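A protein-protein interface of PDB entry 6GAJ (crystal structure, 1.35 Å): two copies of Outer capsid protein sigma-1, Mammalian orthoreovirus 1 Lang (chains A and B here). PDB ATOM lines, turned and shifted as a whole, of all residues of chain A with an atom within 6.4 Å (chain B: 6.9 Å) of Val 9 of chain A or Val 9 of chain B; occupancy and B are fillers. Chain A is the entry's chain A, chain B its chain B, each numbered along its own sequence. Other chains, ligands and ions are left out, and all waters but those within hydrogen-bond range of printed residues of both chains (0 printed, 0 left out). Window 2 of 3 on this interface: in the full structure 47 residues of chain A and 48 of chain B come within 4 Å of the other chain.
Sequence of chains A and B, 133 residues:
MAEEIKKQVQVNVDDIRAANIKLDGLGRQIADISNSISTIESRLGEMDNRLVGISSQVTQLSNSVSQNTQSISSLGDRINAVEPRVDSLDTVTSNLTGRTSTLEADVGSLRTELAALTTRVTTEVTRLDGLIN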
ATOM      1  N   GLU A   4      11.433   4.181 -12.311  1.00  0.00           N
ATOM      2  CA  GLU A   4      10.217   4.105 -11.487  1.00  0.00           C
ATOM      3  C   GLU A   4       9.932   2.639 -11.188  1.00  0.00           C
ATOM      4  O   GLU A   4       9.569   2.322 -10.054  1.00  0.00           O
ATOM      5  CB  GLU A   4       9.010   4.724 -12.225  1.00  0.00           C
ATOM      6  N   ILE A   5      10.136   1.751 -12.180  1.00  0.00           N
ATOM      7  CA  ILE A   5       9.849   0.333 -11.953  1.00  0.00           C
ATOM      8  C   ILE A   5      10.830  -0.230 -10.919  1.00  0.00           C
ATOM      9  O   ILE A   5      10.353  -0.858  -9.940  1.00  0.00           O
ATOM     10  CB  ILE A   5       9.920  -0.475 -13.259  1.00  0.00           C
ATOM     11  CG1 ILE A   5       8.882   0.005 -14.281  1.00  0.00           C
ATOM     12  CG2 ILE A   5       9.706  -1.992 -12.938  1.00  0.00           C
ATOM     13  CD1 ILE A   5       9.229  -0.529 -15.787  1.00  0.00           C
ATOM     14  N   LYS A   6      12.103   0.050 -11.019  1.00  0.00           N
ATOM     15  CA  LYS A   6      13.112  -0.450 -10.112  1.00  0.00           C
ATOM     16  C   LYS A   6      12.750  -0.046  -8.652  1.00  0.00           C
ATOM     17  O   LYS A   6      12.825  -0.866  -7.697  1.00  0.00           O
ATOM     18  CB  LYS A   6      14.467   0.188 -10.489  1.00  0.00           C
ATOM     19  CG  LYS A   6      15.597  -0.438  -9.722  1.00  0.00           C
ATOM     20  CD  LYS A   6      16.912   0.135 -10.233  1.00  0.00           C
ATOM     21  CE  LYS A   6      18.036  -0.146  -9.250  1.00  0.00           C
ATOM     22  NZ  LYS A   6      18.618  -1.509  -9.410  1.00  0.00           N
ATOM     23  N   LYS A   7      12.310   1.224  -8.480  1.00  0.00           N
ATOM     24  CA  LYS A   7      11.955   1.725  -7.154  1.00  0.00           C
ATOM     25  C   LYS A   7      10.718   1.026  -6.567  1.00  0.00           C
ATOM     26  O   LYS A   7      10.700   0.663  -5.366  1.00  0.00           O
ATOM     27  CB  LYS A   7      11.773   3.256  -7.167  1.00  0.00           C
ATOM     28  CG  LYS A   7      13.111   3.948  -7.395  1.00  0.00           C
ATOM     29  CD  LYS A   7      12.950   5.481  -7.431  1.00  0.00           C
ATOM     30  CE  LYS A   7      14.291   6.106  -7.620  1.00  0.00           C
ATOM     31  NZ  LYS A   7      14.082   7.587  -7.776  1.00  0.00           N
ATOM     32  N   GLN A   8       9.703   0.772  -7.427  1.00  0.00           N
ATOM     33  CA  GLN A   8       8.494   0.075  -6.977  1.00  0.00           C
ATOM     34  C   GLN A   8       8.773  -1.361  -6.631  1.00  0.00           C
ATOM     35  O   GLN A   8       8.220  -1.886  -5.665  1.00  0.00           O
ATOM     36  CB  GLN A   8       7.396   0.203  -8.008  1.00  0.00           C
ATOM     37  CG  GLN A   8       6.062  -0.451  -7.566  1.00  0.00           C
ATOM     38  CD  GLN A   8       5.469   0.288  -6.365  1.00  0.00           C
ATOM     39  OE1 GLN A   8       4.937   1.416  -6.504  1.00  0.00           O
ATOM     40  NE2 GLN A   8       5.377  -0.357  -5.229  1.00  0.00           N
ATOM     41  N   VAL A   9       9.688  -1.993  -7.352  1.00  0.00           N
ATOM     42  CA  VAL A   9      10.002  -3.387  -7.029  1.00  0.00           C
ATOM     43  C   VAL A   9      10.668  -3.438  -5.655  1.00  0.00           C
ATOM     44  O   VAL A   9      10.365  -4.349  -4.857  1.00  0.00           O
ATOM     45  CB  VAL A   9      10.904  -3.938  -8.128  1.00  0.00           C
ATOM     46  CG1 VAL A   9      11.525  -5.304  -7.745  1.00  0.00           C
ATOM     47  CG2 VAL A   9      10.108  -4.079  -9.411  1.00  0.00           C
ATOM     48  N   GLN A  10      11.626  -2.493  -5.339  1.00  0.00           N
ATOM     49  CA  GLN A  10      12.253  -2.505  -4.010  1.00  0.00           C
ATOM     50  C   GLN A  10      11.221  -2.136  -2.925  1.00  0.00           C
ATOM     51  O   GLN A  10      11.257  -2.743  -1.868  1.00  0.00           O
ATOM     52  CB  GLN A  10      13.454  -1.525  -3.936  1.00  0.00           C
ATOM     53  CG  GLN A  10      14.181  -1.486  -2.557  1.00  0.00           C
ATOM     54  CD  GLN A  10      14.701  -2.843  -2.114  1.00  0.00           C
ATOM     55  OE1 GLN A  10      15.304  -3.575  -2.890  1.00  0.00           O
ATOM     56  NE2 GLN A  10      14.655  -3.148  -0.801  1.00  0.00           N
ATOM     57  N   VAL A  11      10.239  -1.259  -3.220  1.00  0.00           N
ATOM     58  CA  VAL A  11       9.168  -0.957  -2.234  1.00  0.00           C
ATOM     59  C   VAL A  11       8.393  -2.271  -1.967  1.00  0.00           C
ATOM     60  O   VAL A  11       8.097  -2.565  -0.829  1.00  0.00           O
ATOM     61  CB  VAL A  11       8.221   0.132  -2.776  1.00  0.00           C
ATOM     62  CG1 VAL A  11       6.849   0.106  -2.082  1.00  0.00           C
ATOM     63  CG2 VAL A  11       8.876   1.511  -2.643  1.00  0.00           C
ATOM     64  N   ASN A  12       8.149  -3.056  -3.021  1.00  0.00           N
ATOM     65  CA  ASN A  12       7.439  -4.339  -2.819  1.00  0.00           C
ATOM     66  C   ASN A  12       8.284  -5.301  -1.992  1.00  0.00           C
ATOM     67  O   ASN A  12       7.767  -5.941  -1.092  1.00  0.00           O
ATOM     68  CB  ASN A  12       7.023  -4.956  -4.158  1.00  0.00           C
ATOM     69  CG  ASN A  12       5.863  -4.197  -4.786  1.00  0.00           C
ATOM     70  OD1 ASN A  12       5.261  -3.289  -4.187  1.00  0.00           O
ATOM     71  ND2 ASN A  12       5.559  -4.499  -6.063  1.00  0.00           N
ATOM     72  N   VAL A  13       9.590  -5.336  -2.189  1.00  0.00           N
ATOM     73  CA  VAL A  13      10.467  -6.153  -1.362  1.00  0.00           C
ATOM     74  C   VAL A  13      10.297  -5.709   0.108  1.00  0.00           C
ATOM     75  O   VAL A  13      10.124  -6.519   1.038  1.00  0.00           O
ATOM     76  CB  VAL A  13      11.961  -6.014  -1.787  1.00  0.00           C
ATOM     77  CG1 VAL A  13      12.882  -6.645  -0.777  1.00  0.00           C
ATOM     78  CG2 VAL A  13      12.220  -6.613  -3.184  1.00  0.00           C
ATOM     79  N   ASP A  14      10.335  -4.383   0.316  1.00  0.00           N
ATOM     80  CA  ASP A  14      10.211  -3.826   1.684  1.00  0.00           C
ATOM     81  C   ASP A  14       8.855  -4.172   2.299  1.00  0.00           C
ATOM     82  O   ASP A  14       8.782  -4.487   3.504  1.00  0.00           O
ATOM     83  CB  ASP A  14      10.368  -2.302   1.623  1.00  0.00           C
ATOM     84  CG  ASP A  14      11.776  -1.880   1.241  1.00  0.00           C
ATOM     85  OD1 ASP A  14      12.732  -2.639   1.556  1.00  0.00           O
ATOM     86  OD2 ASP A  14      11.941  -0.704   0.765  1.00  0.00           O
ATOM     87  N   GLU B   4       5.095  -5.958 -19.769  1.00  0.00           N
ATOM     88  CA  GLU B   4       4.778  -7.172 -18.992  1.00  0.00           C
ATOM     89  C   GLU B   4       5.331  -7.052 -17.560  1.00  0.00           C
ATOM     90  O   GLU B   4       4.691  -7.528 -16.608  1.00  0.00           O
ATOM     91  CB  GLU B   4       5.378  -8.430 -19.668  1.00  0.00           C
ATOM     92  N   ILE B   5       6.525  -6.421 -17.410  1.00  0.00           N
ATOM     93  CA  ILE B   5       7.120  -6.254 -16.101  1.00  0.00           C
ATOM     94  C   ILE B   5       6.266  -5.279 -15.279  1.00  0.00           C
ATOM     95  O   ILE B   5       5.877  -5.640 -14.160  1.00  0.00           O
ATOM     96  CB  ILE B   5       8.590  -5.797 -16.186  1.00  0.00           C
ATOM     97  CG1 ILE B   5       9.462  -6.847 -16.960  1.00  0.00           C
ATOM     98  CG2 ILE B   5       9.162  -5.536 -14.757  1.00  0.00           C
ATOM     99  CD1 ILE B   5      11.000  -6.413 -17.212  1.00  0.00           C
ATOM    100  N   LYS B   6       6.013  -4.051 -15.769  1.00  0.00           N
ATOM    101  CA  LYS B   6       5.183  -3.094 -15.013  1.00  0.00           C
ATOM    102  C   LYS B   6       3.843  -3.737 -14.595  1.00  0.00           C
ATOM    103  O   LYS B   6       3.384  -3.566 -13.464  1.00  0.00           O
ATOM    104  CB  LYS B   6       4.913  -1.847 -15.894  1.00  0.00           C
ATOM    105  CG  LYS B   6       4.063  -0.770 -15.237  1.00  0.00           C
ATOM    106  N   LYS B   7       3.177  -4.472 -15.491  1.00  0.00           N
ATOM    107  CA  LYS B   7       1.915  -5.115 -15.162  1.00  0.00           C
ATOM    108  C   LYS B   7       2.047  -6.126 -13.994  1.00  0.00           C
ATOM    109  O   LYS B   7       1.226  -6.118 -13.081  1.00  0.00           O
ATOM    110  CB  LYS B   7       1.255  -5.731 -16.389  1.00  0.00           C
ATOM    111  CG  LYS B   7       0.321  -6.935 -16.081  1.00  0.00           C
ATOM    112  CD  LYS B   7      -0.192  -7.652 -17.330  1.00  0.00           C
ATOM    113  CE  LYS B   7      -1.546  -7.147 -17.753  1.00  0.00           C
ATOM    114  NZ  LYS B   7      -2.472  -8.188 -18.297  1.00  0.00           N
ATOM    115  N   GLN B   8       3.091  -6.977 -14.007  1.00  0.00           N
ATOM    116  CA  GLN B   8       3.268  -7.899 -12.899  1.00  0.00           C
ATOM    117  C   GLN B   8       3.584  -7.140 -11.600  1.00  0.00           C
ATOM    118  O   GLN B   8       3.125  -7.553 -10.515  1.00  0.00           O
ATOM    119  CB  GLN B   8       4.368  -8.919 -13.203  1.00  0.00           C
ATOM    120  CG  GLN B   8       4.491  -9.991 -12.097  1.00  0.00           C
ATOM    121  CD  GLN B   8       3.283 -10.867 -11.915  1.00  0.00           C
ATOM    122  OE1 GLN B   8       2.956 -11.679 -12.797  1.00  0.00           O
ATOM    123  NE2 GLN B   8       2.578 -10.784 -10.797  1.00  0.00           N
ATOM    124  N   VAL B   9       4.360  -6.056 -11.689  1.00  0.00           N
ATOM    125  CA  VAL B   9       4.681  -5.247 -10.517  1.00  0.00           C
ATOM    126  C   VAL B   9       3.400  -4.700  -9.910  1.00  0.00           C
ATOM    127  O   VAL B   9       3.210  -4.733  -8.681  1.00  0.00           O
ATOM    128  CB  VAL B   9       5.651  -4.125 -10.889  1.00  0.00           C
ATOM    129  CG1 VAL B   9       5.906  -3.230  -9.685  1.00  0.00           C
ATOM    130  CG2 VAL B   9       7.000  -4.708 -11.307  1.00  0.00           C
ATOM    131  N   GLN B  10       2.477  -4.201 -10.770  1.00  0.00           N
ATOM    132  CA  GLN B  10       1.214  -3.683 -10.262  1.00  0.00           C
ATOM    133  C   GLN B  10       0.309  -4.748  -9.672  1.00  0.00           C
ATOM    134  O   GLN B  10      -0.316  -4.492  -8.632  1.00  0.00           O
ATOM    135  CB  GLN B  10       0.556  -2.807 -11.332  1.00  0.00           C
ATOM    136  CG  GLN B  10       1.319  -1.450 -11.552  1.00  0.00           C
ATOM    137  CD  GLN B  10       1.601  -0.575 -10.305  1.00  0.00           C
ATOM    138  OE1 GLN B  10       2.727  -0.082 -10.061  1.00  0.00           O
ATOM    139  NE2 GLN B  10       0.569  -0.286  -9.518  1.00  0.00           N
ATOM    140  N   VAL B  11       0.326  -5.969 -10.204  1.00  0.00           N
ATOM    141  CA  VAL B  11      -0.420  -7.087  -9.663  1.00  0.00           C
ATOM    142  C   VAL B  11       0.178  -7.422  -8.242  1.00  0.00           C
ATOM    143  O   VAL B  11      -0.571  -7.656  -7.298  1.00  0.00           O
ATOM    144  CB  VAL B  11      -0.303  -8.337 -10.600  1.00  0.00           C
ATOM    145  CG1 VAL B  11      -0.711  -9.612  -9.876  1.00  0.00           C
ATOM    146  CG2 VAL B  11      -1.165  -8.153 -11.861  1.00  0.00           C
ATOM    147  N   ASN B  12       1.524  -7.393  -8.135  1.00  0.00           N
ATOM    148  CA  ASN B  12       2.164  -7.644  -6.821  1.00  0.00           C
ATOM    149  C   ASN B  12       1.805  -6.536  -5.810  1.00  0.00           C
ATOM    150  O   ASN B  12       1.487  -6.862  -4.674  1.00  0.00           O
ATOM    151  CB  ASN B  12       3.653  -7.741  -7.043  1.00  0.00           C
ATOM    152  CG  ASN B  12       4.085  -9.053  -7.683  1.00  0.00           C
ATOM    153  OD1 ASN B  12       3.259  -9.950  -7.935  1.00  0.00           O
ATOM    154  ND2 ASN B  12       5.377  -9.164  -8.011  1.00  0.00           N
ATOM    155  N   VAL B  13       1.700  -5.288  -6.247  1.00  0.00           N
ATOM    156  CA  VAL B  13       1.275  -4.230  -5.318  1.00  0.00           C
ATOM    157  C   VAL B  13      -0.131  -4.611  -4.799  1.00  0.00           C
ATOM    158  O   VAL B  13      -0.411  -4.577  -3.579  1.00  0.00           O
ATOM    159  CB  VAL B  13       1.250  -2.829  -6.031  1.00  0.00           C
ATOM    160  CG1 VAL B  13       0.639  -1.803  -5.082  1.00  0.00           C
ATOM    161  CG2 VAL B  13       2.654  -2.367  -6.430  1.00  0.00           C
ATOM    162  N   ASP B  14      -1.056  -4.995  -5.708  1.00  0.00           N
ATOM    163  CA  ASP B  14      -2.402  -5.371  -5.308  1.00  0.00           C
ATOM    164  C   ASP B  14      -2.455  -6.566  -4.334  1.00  0.00           C
ATOM    165  O   ASP B  14      -3.189  -6.568  -3.328  1.00  0.00           O
ATOM    166  CB  ASP B  14      -3.213  -5.689  -6.573  1.00  0.00           C
ATOM    167  CG  ASP B  14      -4.678  -5.695  -6.256  1.00  0.00           C
ATOM    168  OD1 ASP B  14      -5.209  -4.622  -5.898  1.00  0.00           O
ATOM    169  OD2 ASP B  14      -5.279  -6.785  -6.246  1.00  0.00           O
ATOM    170  N   ILE B  16      -0.067  -7.638  -2.364  1.00  0.00           N
ATOM    171  CA  ILE B  16       0.483  -7.272  -1.054  1.00  0.00           C
ATOM    172  C   ILE B  16      -0.622  -6.540  -0.251  1.00  0.00           C
ATOM    173  O   ILE B  16      -0.795  -6.795   0.971  1.00  0.00           O
ATOM    174  CB  ILE B  16       1.758  -6.435  -1.215  1.00  0.00           C
ATOM    175  CG1 ILE B  16       2.892  -7.276  -1.822  1.00  0.00           C
ATOM    176  CG2 ILE B  16       2.180  -5.749   0.126  1.00  0.00           C
ATOM    177  CD1 ILE B  16       4.045  -6.438  -2.442  1.00  0.00           C
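Of the 12 printed residues of chain B, 4 touch a printed residue of chain A.
Printed residues of chain B that touch a printed residue of chain A: Val 9, Asn 12, Val 13 and Ile 16.
Among the printed residues, 7 pairs touch across the chains.
Among the printed residues, no Asp or Glu carboxylate lies within 4 Å of a Lys or Arg side-chain nitrogen of the other chain.
Gln 8 of chain A touches Val 9 of chain B, but with the chains exchanged Val 9 of chain A does not touch Gln 8 of chain B (7.5 Å).
Gln 8 of chain A touches Val 13 of chain B, but with the chains exchanged Val 13 of chain A does not touch Gln 8 of chain B (10.8 Å).
Val 9 of chain A touches its own counterpart, Val 9 of chain B.
Asn 12 of chain A touches Val 13 of chain B, but with the chains exchanged Val 13 of chain A does not touch Asn 12 of chain B (8.0 Å).
Positions printed for both chains: 4, 5, 6, 7, 8, 9, 10, 11, 12, 13 and 14.
Of the 7 pairs that touch across the chains among the printed residues, 2 have their exchanged pair printed and touching as well.
Of chain B, only Val 9 comes within 4 Å of Val 9 of chain A.
Of the printed residues of chain B, Asn 12 of chain A touches Val 9, Asn 12, Val 13 and Ile 16.
Val 13 of chain A touches none of the printed residues of chain B.
Asp 14 of chain A touches none of the printed residues of chain B.
Val 9 of chain B touches just these residues of chain A: Gln 8 (3.5 Å), Val 9 (3.7 Å) and Asn 12 (3.5 Å).
Of the printed residues of chain A, Asn 12 of chain B touches Asn 12 (3.9 Å).
Of the printed residues of chain A, Val 13 of chain B touches Gln 8 (3.6 Å) and Asn 12 (3.6 Å).
Printed residues of chain A within 4 Å of Ile 16 of chain B: Asn 12.
The nearest printed residue of chain A that does not touch Ile 16 of chain B is Val 13 of chain A (5.7 Å).
CG of Gln 8 of chain A touches CG1 of Val 9 of chain B (3.5 Å).
Gln 8 of chain A touches Val 13 of chain B (NE2 to CG2, 3.6 Å).
Val 9 of chain A touches Val 9 of chain B.
Asn 12 of chain A touches Val 9 of chain B (ND2 to O, 3.5 Å).
Asn 12 of chain A touches Asn 12 of chain B (ND2 to CB, 3.9 Å).
OD1 of Asn 12 of chain A touches CG2 of Val 13 of chain B (3.6 Å).
Asn 12 of chain A touches Ile 16 of chain B.
The side-chain amide oxygen (OD1) of Asn 12 of chain A lies within hydrogen-bond range of the side-chain amide nitrogen (NE2) of Gln 8 of chain A, 3.1 Å away.
The side-chain amide oxygen (OD1) of Asn 12 of chain B sits at hydrogen-bond distance from the side-chain amide nitrogen (NE2) of Gln 8 of chain B.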
